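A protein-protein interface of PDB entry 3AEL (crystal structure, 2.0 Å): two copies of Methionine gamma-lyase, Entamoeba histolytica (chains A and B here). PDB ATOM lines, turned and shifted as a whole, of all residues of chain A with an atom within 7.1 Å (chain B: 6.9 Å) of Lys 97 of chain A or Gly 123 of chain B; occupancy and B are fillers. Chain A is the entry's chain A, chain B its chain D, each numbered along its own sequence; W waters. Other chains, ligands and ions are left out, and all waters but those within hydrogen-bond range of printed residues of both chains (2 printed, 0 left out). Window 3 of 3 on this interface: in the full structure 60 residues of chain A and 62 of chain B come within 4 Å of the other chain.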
ATOM      1  N   LEU A  95       1.821   2.583 -11.135  1.00  0.00           N
ATOM      2  CA  LEU A  95       0.888   1.650 -11.773  1.00  0.00           C
ATOM      3  C   LEU A  95       1.432   0.234 -11.658  1.00  0.00           C
ATOM      4  O   LEU A  95       2.633   0.000 -11.854  1.00  0.00           O
ATOM      5  CB  LEU A  95       0.655   2.012 -13.246  1.00  0.00           C
ATOM      6  CG  LEU A  95      -0.004   3.378 -13.507  1.00  0.00           C
ATOM      7  CD1 LEU A  95       0.187   3.753 -14.963  1.00  0.00           C
ATOM      8  CD2 LEU A  95      -1.489   3.265 -13.154  1.00  0.00           C
ATOM      9  N   GLN A  96       0.558  -0.714 -11.339  1.00  0.00           N
ATOM     10  CA  GLN A  96       0.966  -2.115 -11.335  1.00  0.00           C
ATOM     11  C   GLN A  96      -0.067  -2.972 -12.054  1.00  0.00           C
ATOM     12  O   GLN A  96      -1.115  -2.474 -12.483  1.00  0.00           O
ATOM     13  CB  GLN A  96       1.176  -2.609  -9.892  1.00  0.00           C
ATOM     14  CG  GLN A  96      -0.076  -2.592  -9.034  1.00  0.00           C
ATOM     15  CD  GLN A  96       0.241  -2.894  -7.576  1.00  0.00           C
ATOM     16  OE1 GLN A  96       0.687  -3.994  -7.240  1.00  0.00           O
ATOM     17  NE2 GLN A  96       0.025  -1.906  -6.705  1.00  0.00           N
ATOM     18  N   LYS A  97       0.263  -4.249 -12.222  1.00  0.00           N
ATOM     19  CA  LYS A  97      -0.577  -5.182 -12.935  1.00  0.00           C
ATOM     20  C   LYS A  97      -2.011  -5.102 -12.363  1.00  0.00           C
ATOM     21  O   LYS A  97      -2.207  -5.099 -11.145  1.00  0.00           O
ATOM     22  CB  LYS A  97      -0.008  -6.583 -12.773  1.00  0.00           C
ATOM     23  CG  LYS A  97      -0.958  -7.700 -13.233  1.00  0.00           C
ATOM     24  CD  LYS A  97      -0.647  -9.052 -12.554  1.00  0.00           C
ATOM     25  CE  LYS A  97      -0.320  -8.909 -11.030  1.00  0.00           C
ATOM     26  NZ  LYS A  97      -0.354 -10.258 -10.314  1.00  0.00           N
ATOM     27  N   GLY A  98      -3.003  -5.018 -13.236  1.00  0.00           N
ATOM     28  CA  GLY A  98      -4.395  -4.928 -12.752  1.00  0.00           C
ATOM     29  C   GLY A  98      -4.901  -3.492 -12.687  1.00  0.00           C
ATOM     30  O   GLY A  98      -6.113  -3.269 -12.651  1.00  0.00           O
ATOM     31  N   ASP A  99      -3.985  -2.510 -12.689  1.00  0.00           N
ATOM     32  CA  ASP A  99      -4.384  -1.087 -12.709  1.00  0.00           C
ATOM     33  C   ASP A  99      -4.782  -0.645 -14.137  1.00  0.00           C
ATOM     34  O   ASP A  99      -4.402  -1.275 -15.150  1.00  0.00           O
ATOM     35  CB  ASP A  99      -3.240  -0.178 -12.203  1.00  0.00           C
ATOM     36  CG  ASP A  99      -2.969  -0.342 -10.698  1.00  0.00           C
ATOM     37  OD1 ASP A  99      -1.893   0.137 -10.234  1.00  0.00           O
ATOM     38  OD2 ASP A  99      -3.808  -0.948  -9.977  1.00  0.00           O
ATOM     39  N   HIS A 100      -5.500   0.463 -14.212  1.00  0.00           N
ATOM     40  CA  HIS A 100      -5.912   1.034 -15.492  1.00  0.00           C
ATOM     41  C   HIS A 100      -5.452   2.491 -15.584  1.00  0.00           C
ATOM     42  O   HIS A 100      -5.509   3.244 -14.606  1.00  0.00           O
ATOM     43  CB  HIS A 100      -7.434   0.833 -15.646  1.00  0.00           C
ATOM     44  CG  HIS A 100      -8.104   1.649 -16.715  1.00  0.00           C
ATOM     45  ND1 HIS A 100      -7.911   1.438 -18.069  1.00  0.00           N
ATOM     46  CD2 HIS A 100      -9.061   2.601 -16.623  1.00  0.00           C
ATOM     47  CE1 HIS A 100      -8.699   2.243 -18.764  1.00  0.00           C
ATOM     48  NE2 HIS A 100      -9.415   2.957 -17.906  1.00  0.00           N
ATOM     49  N   LEU A 119       3.637  -0.751 -21.239  1.00  0.00           N
ATOM     50  CA  LEU A 119       2.675  -0.898 -20.120  1.00  0.00           C
ATOM     51  C   LEU A 119       1.793  -2.164 -20.155  1.00  0.00           C
ATOM     52  O   LEU A 119       1.691  -2.858 -19.140  1.00  0.00           O
ATOM     53  CB  LEU A 119       1.851   0.382 -19.917  1.00  0.00           C
ATOM     54  CG  LEU A 119       2.452   1.400 -18.934  1.00  0.00           C
ATOM     55  CD1 LEU A 119       3.859   1.976 -19.334  1.00  0.00           C
ATOM     56  CD2 LEU A 119       1.422   2.531 -18.713  1.00  0.00           C
ATOM     57  N   ARG A 121       2.516  -4.978 -21.414  1.00  0.00           N
ATOM     58  CA  ARG A 121       3.353  -6.158 -21.150  1.00  0.00           C
ATOM     59  C   ARG A 121       3.511  -6.362 -19.642  1.00  0.00           C
ATOM     60  O   ARG A 121       3.818  -7.452 -19.194  1.00  0.00           O
ATOM     61  CB  ARG A 121       4.729  -6.011 -21.806  1.00  0.00           C
ATOM     62  CG  ARG A 121       4.684  -6.130 -23.314  1.00  0.00           C
ATOM     63  CD  ARG A 121       6.027  -5.749 -23.949  1.00  0.00           C
ATOM     64  NE  ARG A 121       7.118  -6.662 -23.586  1.00  0.00           N
ATOM     65  CZ  ARG A 121       7.380  -7.821 -24.192  1.00  0.00           C
ATOM     66  NH1 ARG A 121       6.618  -8.268 -25.200  1.00  0.00           N
ATOM     67  NH2 ARG A 121       8.393  -8.564 -23.768  1.00  0.00           N
ATOM     68  N   PHE A 122       3.305  -5.293 -18.878  1.00  0.00           N
ATOM     69  CA  PHE A 122       3.391  -5.310 -17.419  1.00  0.00           C
ATOM     70  C   PHE A 122       2.000  -5.435 -16.753  1.00  0.00           C
ATOM     71  O   PHE A 122       1.874  -5.239 -15.540  1.00  0.00           O
ATOM     72  CB  PHE A 122       4.145  -4.053 -16.930  1.00  0.00           C
ATOM     73  CG  PHE A 122       5.543  -3.898 -17.528  1.00  0.00           C
ATOM     74  CD1 PHE A 122       6.091  -2.621 -17.746  1.00  0.00           C
ATOM     75  CD2 PHE A 122       6.303  -5.021 -17.884  1.00  0.00           C
ATOM     76  CE1 PHE A 122       7.384  -2.477 -18.306  1.00  0.00           C
ATOM     77  CE2 PHE A 122       7.567  -4.872 -18.451  1.00  0.00           C
ATOM     78  CZ  PHE A 122       8.102  -3.581 -18.647  1.00  0.00           C
ATOM     79  N   GLY A 123       0.981  -5.758 -17.563  1.00  0.00           N
ATOM     80  CA  GLY A 123      -0.334  -6.161 -17.093  1.00  0.00           C
ATOM     81  C   GLY A 123      -1.137  -4.945 -16.691  1.00  0.00           C
ATOM     82  O   GLY A 123      -2.109  -5.051 -15.949  1.00  0.00           O
ATOM     83  N   ILE A 124      -0.725  -3.782 -17.196  1.00  0.00           N
ATOM     84  CA  ILE A 124      -1.428  -2.522 -16.952  1.00  0.00           C
ATOM     85  C   ILE A 124      -2.325  -2.250 -18.160  1.00  0.00           C
ATOM     86  O   ILE A 124      -1.861  -2.308 -19.303  1.00  0.00           O
ATOM     87  CB  ILE A 124      -0.427  -1.355 -16.771  1.00  0.00           C
ATOM     88  CG1 ILE A 124       0.491  -1.639 -15.562  1.00  0.00           C
ATOM     89  CG2 ILE A 124      -1.151  -0.002 -16.583  1.00  0.00           C
ATOM     90  CD1 ILE A 124       1.768  -0.740 -15.536  1.00  0.00           C
ATOM     91  N   GLU A 125      -3.601  -1.982 -17.894  1.00  0.00           N
ATOM     92  CA  GLU A 125      -4.587  -1.683 -18.907  1.00  0.00           C
ATOM     93  C   GLU A 125      -4.530  -0.215 -19.268  1.00  0.00           C
ATOM     94  O   GLU A 125      -4.458   0.647 -18.391  1.00  0.00           O
ATOM     95  CB  GLU A 125      -6.006  -2.049 -18.413  1.00  0.00           C
ATOM     96  CG  GLU A 125      -6.126  -3.479 -17.897  1.00  0.00           C
ATOM     97  CD  GLU A 125      -7.443  -3.745 -17.127  1.00  0.00           C
ATOM     98  OE1 GLU A 125      -8.235  -2.831 -16.886  1.00  0.00           O
ATOM     99  OE2 GLU A 125      -7.694  -4.890 -16.763  1.00  0.00           O
ATOM    100  N   ASN A 144     -11.019   0.092 -11.571  1.00  0.00           N
ATOM    101  CA  ASN A 144      -9.575  -0.034 -11.324  1.00  0.00           C
ATOM    102  C   ASN A 144      -8.724   1.105 -11.951  1.00  0.00           C
ATOM    103  O   ASN A 144      -7.472   1.031 -11.978  1.00  0.00           O
ATOM    104  CB  ASN A 144      -9.085  -1.423 -11.808  1.00  0.00           C
ATOM    105  CG  ASN A 144      -9.252  -1.602 -13.331  1.00  0.00           C
ATOM    106  OD1 ASN A 144     -10.265  -1.168 -13.904  1.00  0.00           O
ATOM    107  ND2 ASN A 144      -8.265  -2.244 -13.986  1.00  0.00           N
ATOM    108  N   GLN B  96       7.800 -10.233 -19.342  1.00  0.00           N
ATOM    109  CA  GLN B  96       6.433  -9.657 -19.274  1.00  0.00           C
ATOM    110  C   GLN B  96       5.557 -10.459 -18.300  1.00  0.00           C
ATOM    111  O   GLN B  96       5.977 -11.521 -17.818  1.00  0.00           O
ATOM    112  CB  GLN B  96       5.784  -9.585 -20.664  1.00  0.00           C
ATOM    113  CG  GLN B  96       5.509 -10.933 -21.345  1.00  0.00           C
ATOM    114  CD  GLN B  96       5.030 -10.765 -22.783  1.00  0.00           C
ATOM    115  OE1 GLN B  96       4.002 -10.147 -23.039  1.00  0.00           O
ATOM    116  NE2 GLN B  96       5.777 -11.325 -23.726  1.00  0.00           N
ATOM    117  N   LYS B  97       4.379  -9.918 -17.992  1.00  0.00           N
ATOM    118  CA  LYS B  97       3.391 -10.551 -17.131  1.00  0.00           C
ATOM    119  C   LYS B  97       3.242 -12.022 -17.527  1.00  0.00           C
ATOM    120  O   LYS B  97       3.009 -12.325 -18.693  1.00  0.00           O
ATOM    121  CB  LYS B  97       2.037  -9.830 -17.286  1.00  0.00           C
ATOM    122  CG  LYS B  97       0.825 -10.588 -16.740  1.00  0.00           C
ATOM    123  CD  LYS B  97      -0.441  -9.760 -16.919  1.00  0.00           C
ATOM    124  CE  LYS B  97      -1.709 -10.608 -17.134  1.00  0.00           C
ATOM    125  NZ  LYS B  97      -2.877  -9.677 -17.376  1.00  0.00           N
ATOM    126  N   GLY B  98       3.388 -12.912 -16.552  1.00  0.00           N
ATOM    127  CA  GLY B  98       3.224 -14.343 -16.791  1.00  0.00           C
ATOM    128  C   GLY B  98       4.535 -15.083 -16.913  1.00  0.00           C
ATOM    129  O   GLY B  98       4.549 -16.306 -16.871  1.00  0.00           O
ATOM    130  N   ASP B  99       5.627 -14.341 -17.093  1.00  0.00           N
ATOM    131  CA  ASP B  99       6.964 -14.903 -17.157  1.00  0.00           C
ATOM    132  C   ASP B  99       7.530 -15.153 -15.772  1.00  0.00           C
ATOM    133  O   ASP B  99       7.068 -14.597 -14.782  1.00  0.00           O
ATOM    134  CB  ASP B  99       7.936 -13.984 -17.903  1.00  0.00           C
ATOM    135  CG  ASP B  99       7.663 -13.907 -19.395  1.00  0.00           C
ATOM    136  OD1 ASP B  99       8.288 -13.040 -20.039  1.00  0.00           O
ATOM    137  OD2 ASP B  99       6.832 -14.679 -19.935  1.00  0.00           O
ATOM    138  N   HIS B 100       8.551 -15.999 -15.726  1.00  0.00           N
ATOM    139  CA  HIS B 100       9.220 -16.368 -14.500  1.00  0.00           C
ATOM    140  C   HIS B 100      10.705 -16.083 -14.708  1.00  0.00           C
ATOM    141  O   HIS B 100      11.246 -16.365 -15.775  1.00  0.00           O
ATOM    142  CB  HIS B 100       8.951 -17.861 -14.228  1.00  0.00           C
ATOM    143  CG  HIS B 100       9.776 -18.456 -13.124  1.00  0.00           C
ATOM    144  ND1 HIS B 100       9.755 -17.979 -11.832  1.00  0.00           N
ATOM    145  CD2 HIS B 100      10.607 -19.521 -13.112  1.00  0.00           C
ATOM    146  CE1 HIS B 100      10.561 -18.704 -11.079  1.00  0.00           C
ATOM    147  NE2 HIS B 100      11.088 -19.651 -11.830  1.00  0.00           N
ATOM    148  N   TRP B 118       9.821  -4.317  -7.725  1.00  0.00           N
ATOM    149  CA  TRP B 118       9.192  -3.847  -8.980  1.00  0.00           C
ATOM    150  C   TRP B 118       8.695  -4.949  -9.925  1.00  0.00           C
ATOM    151  O   TRP B 118       7.567  -4.891 -10.402  1.00  0.00           O
ATOM    152  CB  TRP B 118      10.091  -2.843  -9.733  1.00  0.00           C
ATOM    153  CG  TRP B 118      10.364  -1.616  -8.892  1.00  0.00           C
ATOM    154  CD1 TRP B 118      11.550  -1.284  -8.297  1.00  0.00           C
ATOM    155  CD2 TRP B 118       9.435  -0.574  -8.546  1.00  0.00           C
ATOM    156  NE1 TRP B 118      11.422  -0.112  -7.587  1.00  0.00           N
ATOM    157  CE2 TRP B 118      10.134   0.346  -7.716  1.00  0.00           C
ATOM    158  CE3 TRP B 118       8.073  -0.342  -8.826  1.00  0.00           C
ATOM    159  CZ2 TRP B 118       9.532   1.491  -7.183  1.00  0.00           C
ATOM    160  CZ3 TRP B 118       7.464   0.803  -8.281  1.00  0.00           C
ATOM    161  CH2 TRP B 118       8.210   1.712  -7.462  1.00  0.00           C
ATOM    162  N   LEU B 119       9.551  -5.924 -10.210  1.00  0.00           N
ATOM    163  CA  LEU B 119       9.185  -6.996 -11.128  1.00  0.00           C
ATOM    164  C   LEU B 119       7.869  -7.680 -10.789  1.00  0.00           C
ATOM    165  O   LEU B 119       7.048  -7.851 -11.675  1.00  0.00           O
ATOM    166  CB  LEU B 119      10.327  -8.017 -11.280  1.00  0.00           C
ATOM    167  CG  LEU B 119      11.217  -7.705 -12.487  1.00  0.00           C
ATOM    168  CD1 LEU B 119      11.892  -6.327 -12.400  1.00  0.00           C
ATOM    169  CD2 LEU B 119      12.261  -8.805 -12.645  1.00  0.00           C
ATOM    170  N   PRO B 120       7.629  -8.026  -9.508  1.00  0.00           N
ATOM    171  CA  PRO B 120       6.335  -8.646  -9.186  1.00  0.00           C
ATOM    172  C   PRO B 120       5.133  -7.733  -9.362  1.00  0.00           C
ATOM    173  O   PRO B 120       4.049  -8.215  -9.627  1.00  0.00           O
ATOM    174  CB  PRO B 120       6.484  -9.041  -7.711  1.00  0.00           C
ATOM    175  CG  PRO B 120       7.971  -9.281  -7.549  1.00  0.00           C
ATOM    176  CD  PRO B 120       8.568  -8.132  -8.372  1.00  0.00           C
ATOM    177  N   ARG B 121       5.315  -6.428  -9.243  1.00  0.00           N
ATOM    178  CA  ARG B 121       4.230  -5.487  -9.514  1.00  0.00           C
ATOM    179  C   ARG B 121       3.827  -5.508 -11.006  1.00  0.00           C
ATOM    180  O   ARG B 121       2.712  -5.092 -11.394  1.00  0.00           O
ATOM    181  CB  ARG B 121       4.689  -4.080  -9.113  1.00  0.00           C
ATOM    182  CG  ARG B 121       4.776  -3.916  -7.611  1.00  0.00           C
ATOM    183  CD  ARG B 121       5.382  -2.570  -7.205  1.00  0.00           C
ATOM    184  NE  ARG B 121       4.629  -1.388  -7.611  1.00  0.00           N
ATOM    185  CZ  ARG B 121       3.658  -0.809  -6.907  1.00  0.00           C
ATOM    186  NH1 ARG B 121       3.047   0.284  -7.371  1.00  0.00           N
ATOM    187  NH2 ARG B 121       3.270  -1.317  -5.742  1.00  0.00           N
ATOM    188  N   PHE B 122       4.745  -5.976 -11.838  1.00  0.00           N
ATOM    189  CA  PHE B 122       4.525  -6.042 -13.274  1.00  0.00           C
ATOM    190  C   PHE B 122       4.139  -7.463 -13.722  1.00  0.00           C
ATOM    191  O   PHE B 122       4.204  -7.767 -14.917  1.00  0.00           O
ATOM    192  CB  PHE B 122       5.762  -5.536 -14.042  1.00  0.00           C
ATOM    193  CG  PHE B 122       6.168  -4.121 -13.688  1.00  0.00           C
ATOM    194  CD1 PHE B 122       7.516  -3.768 -13.611  1.00  0.00           C
ATOM    195  CD2 PHE B 122       5.189  -3.135 -13.451  1.00  0.00           C
ATOM    196  CE1 PHE B 122       7.928  -2.453 -13.272  1.00  0.00           C
ATOM    197  CE2 PHE B 122       5.576  -1.821 -13.106  1.00  0.00           C
ATOM    198  CZ  PHE B 122       6.962  -1.481 -13.027  1.00  0.00           C
ATOM    199  N   GLY B 123       3.748  -8.303 -12.750  1.00  0.00           N
ATOM    200  CA  GLY B 123       3.223  -9.655 -13.001  1.00  0.00           C
ATOM    201  C   GLY B 123       4.298 -10.674 -13.337  1.00  0.00           C
ATOM    202  O   GLY B 123       4.011 -11.722 -13.883  1.00  0.00           O
ATOM    203  N   ILE B 124       5.546 -10.361 -13.010  1.00  0.00           N
ATOM    204  CA  ILE B 124       6.688 -11.246 -13.299  1.00  0.00           C
ATOM    205  C   ILE B 124       7.058 -12.032 -12.041  1.00  0.00           C
ATOM    206  O   ILE B 124       7.365 -11.440 -10.995  1.00  0.00           O
ATOM    207  CB  ILE B 124       7.899 -10.432 -13.829  1.00  0.00           C
ATOM    208  CG1 ILE B 124       7.496  -9.632 -15.092  1.00  0.00           C
ATOM    209  CG2 ILE B 124       9.134 -11.352 -14.058  1.00  0.00           C
ATOM    210  CD1 ILE B 124       8.476  -8.504 -15.476  1.00  0.00           C
ATOM    211  N   GLU B 125       7.002 -13.356 -12.138  1.00  0.00           N
ATOM    212  CA  GLU B 125       7.317 -14.237 -11.012  1.00  0.00           C
ATOM    213  C   GLU B 125       8.823 -14.297 -10.886  1.00  0.00           C
ATOM    214  O   GLU B 125       9.521 -14.477 -11.887  1.00  0.00           O
ATOM    215  CB  GLU B 125       6.763 -15.661 -11.246  1.00  0.00           C
ATOM    216  CG  GLU B 125       5.239 -15.734 -11.450  1.00  0.00           C
ATOM    217  CD  GLU B 125       4.737 -17.066 -12.049  1.00  0.00           C
ATOM    218  OE1 GLU B 125       3.512 -17.166 -12.260  1.00  0.00           O
ATOM    219  OE2 GLU B 125       5.535 -18.001 -12.320  1.00  0.00           O
HETATM  220  O   HOH W   1       4.519   0.198  -9.917  1.00  0.00           O
HETATM  221  O   HOH W   2      -3.722  -7.281 -15.922  1.00  0.00           O
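The guanidinium group (NH2) of Arg 121 of chain B sits close to the side-chain amide nitrogen (NE2) of Gln 96 of chain A (3.4 Å). N of Lys 97 of chain A lies within hydrogen-bond range of O of Arg 121 of chain B (2.7 Å). NE2 of Gln 96 of chain B lies close to NH1 of Arg 121 of chain A, 3.5 Å away. The backbone NH (N) of Lys 97 of chain B sits at hydrogen-bond distance from the backbone carbonyl oxygen (O) of Arg 121 of chain A, at 2.8 Å. The backbone carbonyl oxygen (O) of Phe 122 of chain B sits close to the backbone carbonyl oxygen (O) of Phe 122 of chain A.
The side-chain carboxylate (OD1) of Asp 99 of chain A lies within hydrogen-bond range of the backbone NH (N) of Gln 96 of chain A (2.8 Å). N of Gly 98 of chain A sits at hydrogen-bond distance from O of Gly 123 of chain A (2.9 Å). The side-chain carboxylate (OD1) of Asp 99 of chain B sits at hydrogen-bond distance from the backbone NH (N) of Gln 96 of chain B (2.9 Å). The backbone NH (N) of Gly 98 of chain B is in hydrogen-bond range of the backbone carbonyl oxygen (O) of Gly 123 of chain B.
CE2 of Phe 122 of chain B touches O of Leu 95 of chain A, at 3.7 Å. Lys 97 of chain A touches Gly 123 of chain B. Lys 97 of chain B touches Gly 123 of chain A (CD to CA, 3.6 Å).
Lys 97 of chain A touches just these residues of chain B: Arg 121 (2.7 Å) and Gly 123 (3.9 Å). Of chain A, only Lys 97 (3.9 Å) comes within 4 Å of Gly 123 of chain B. Of the printed residues of chain B, Leu 95 of chain A touches Phe 122. Printed residues of chain B within 4 Å of Gly 123 of chain A: Lys 97. Printed residues of chain A within 4 Å of Phe 122 of chain B: Leu 95 and Phe 122. Printed residues of chain A within 4 Å of Arg 121 of chain B: Gln 96 (3.3 Å) and Lys 97 (2.7 Å). Asn 144 of chain A touches none of the printed residues of chain B. The nearest residue of chain B that does not touch Lys 97 of chain A is Lys 97 of chain B (4.3 Å). The nearest printed residue of chain A that does not touch Gln 96 of chain B is Phe 122 of chain A (4.8 Å).
Along chain B the printed residues that touch a printed residue of chain A span positions 96 to 123. Hydrophobic or aromatic side chains of chain A within 4 Å of the printed part of chain B: Phe 122. Along chain A the printed residues that touch a printed residue of chain B span positions 95 to 123.
Gln 96 of chain A touches Arg 121 of chain B, and with the chains exchanged Arg 121 of chain A touches Gln 96 of chain B. Lys 97 of chain A touches Arg 121 of chain B, and with the chains exchanged Arg 121 of chain A touches Lys 97 of chain B. Lys 97 of chain A touches Gly 123 of chain B, and with the chains exchanged Gly 123 of chain A touches Lys 97 of chain B. Phe 122 of chain A touches its own counterpart, Phe 122 of chain B. Of the 8 pairs that touch across the chains among the printed residues, 7 have their exchanged pair printed and touching as well.
Water W1 lies within hydrogen-bond range of the backbone carbonyl oxygen of Leu 95 of chain A (2.7 Å) and the guanidinium group of Arg 121 of chain B (2.8 Å). Water W2 lies within hydrogen-bond range of O of Gly 123 of chain A (2.8 Å) and NZ of Lys 97 of chain B (2.9 Å).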
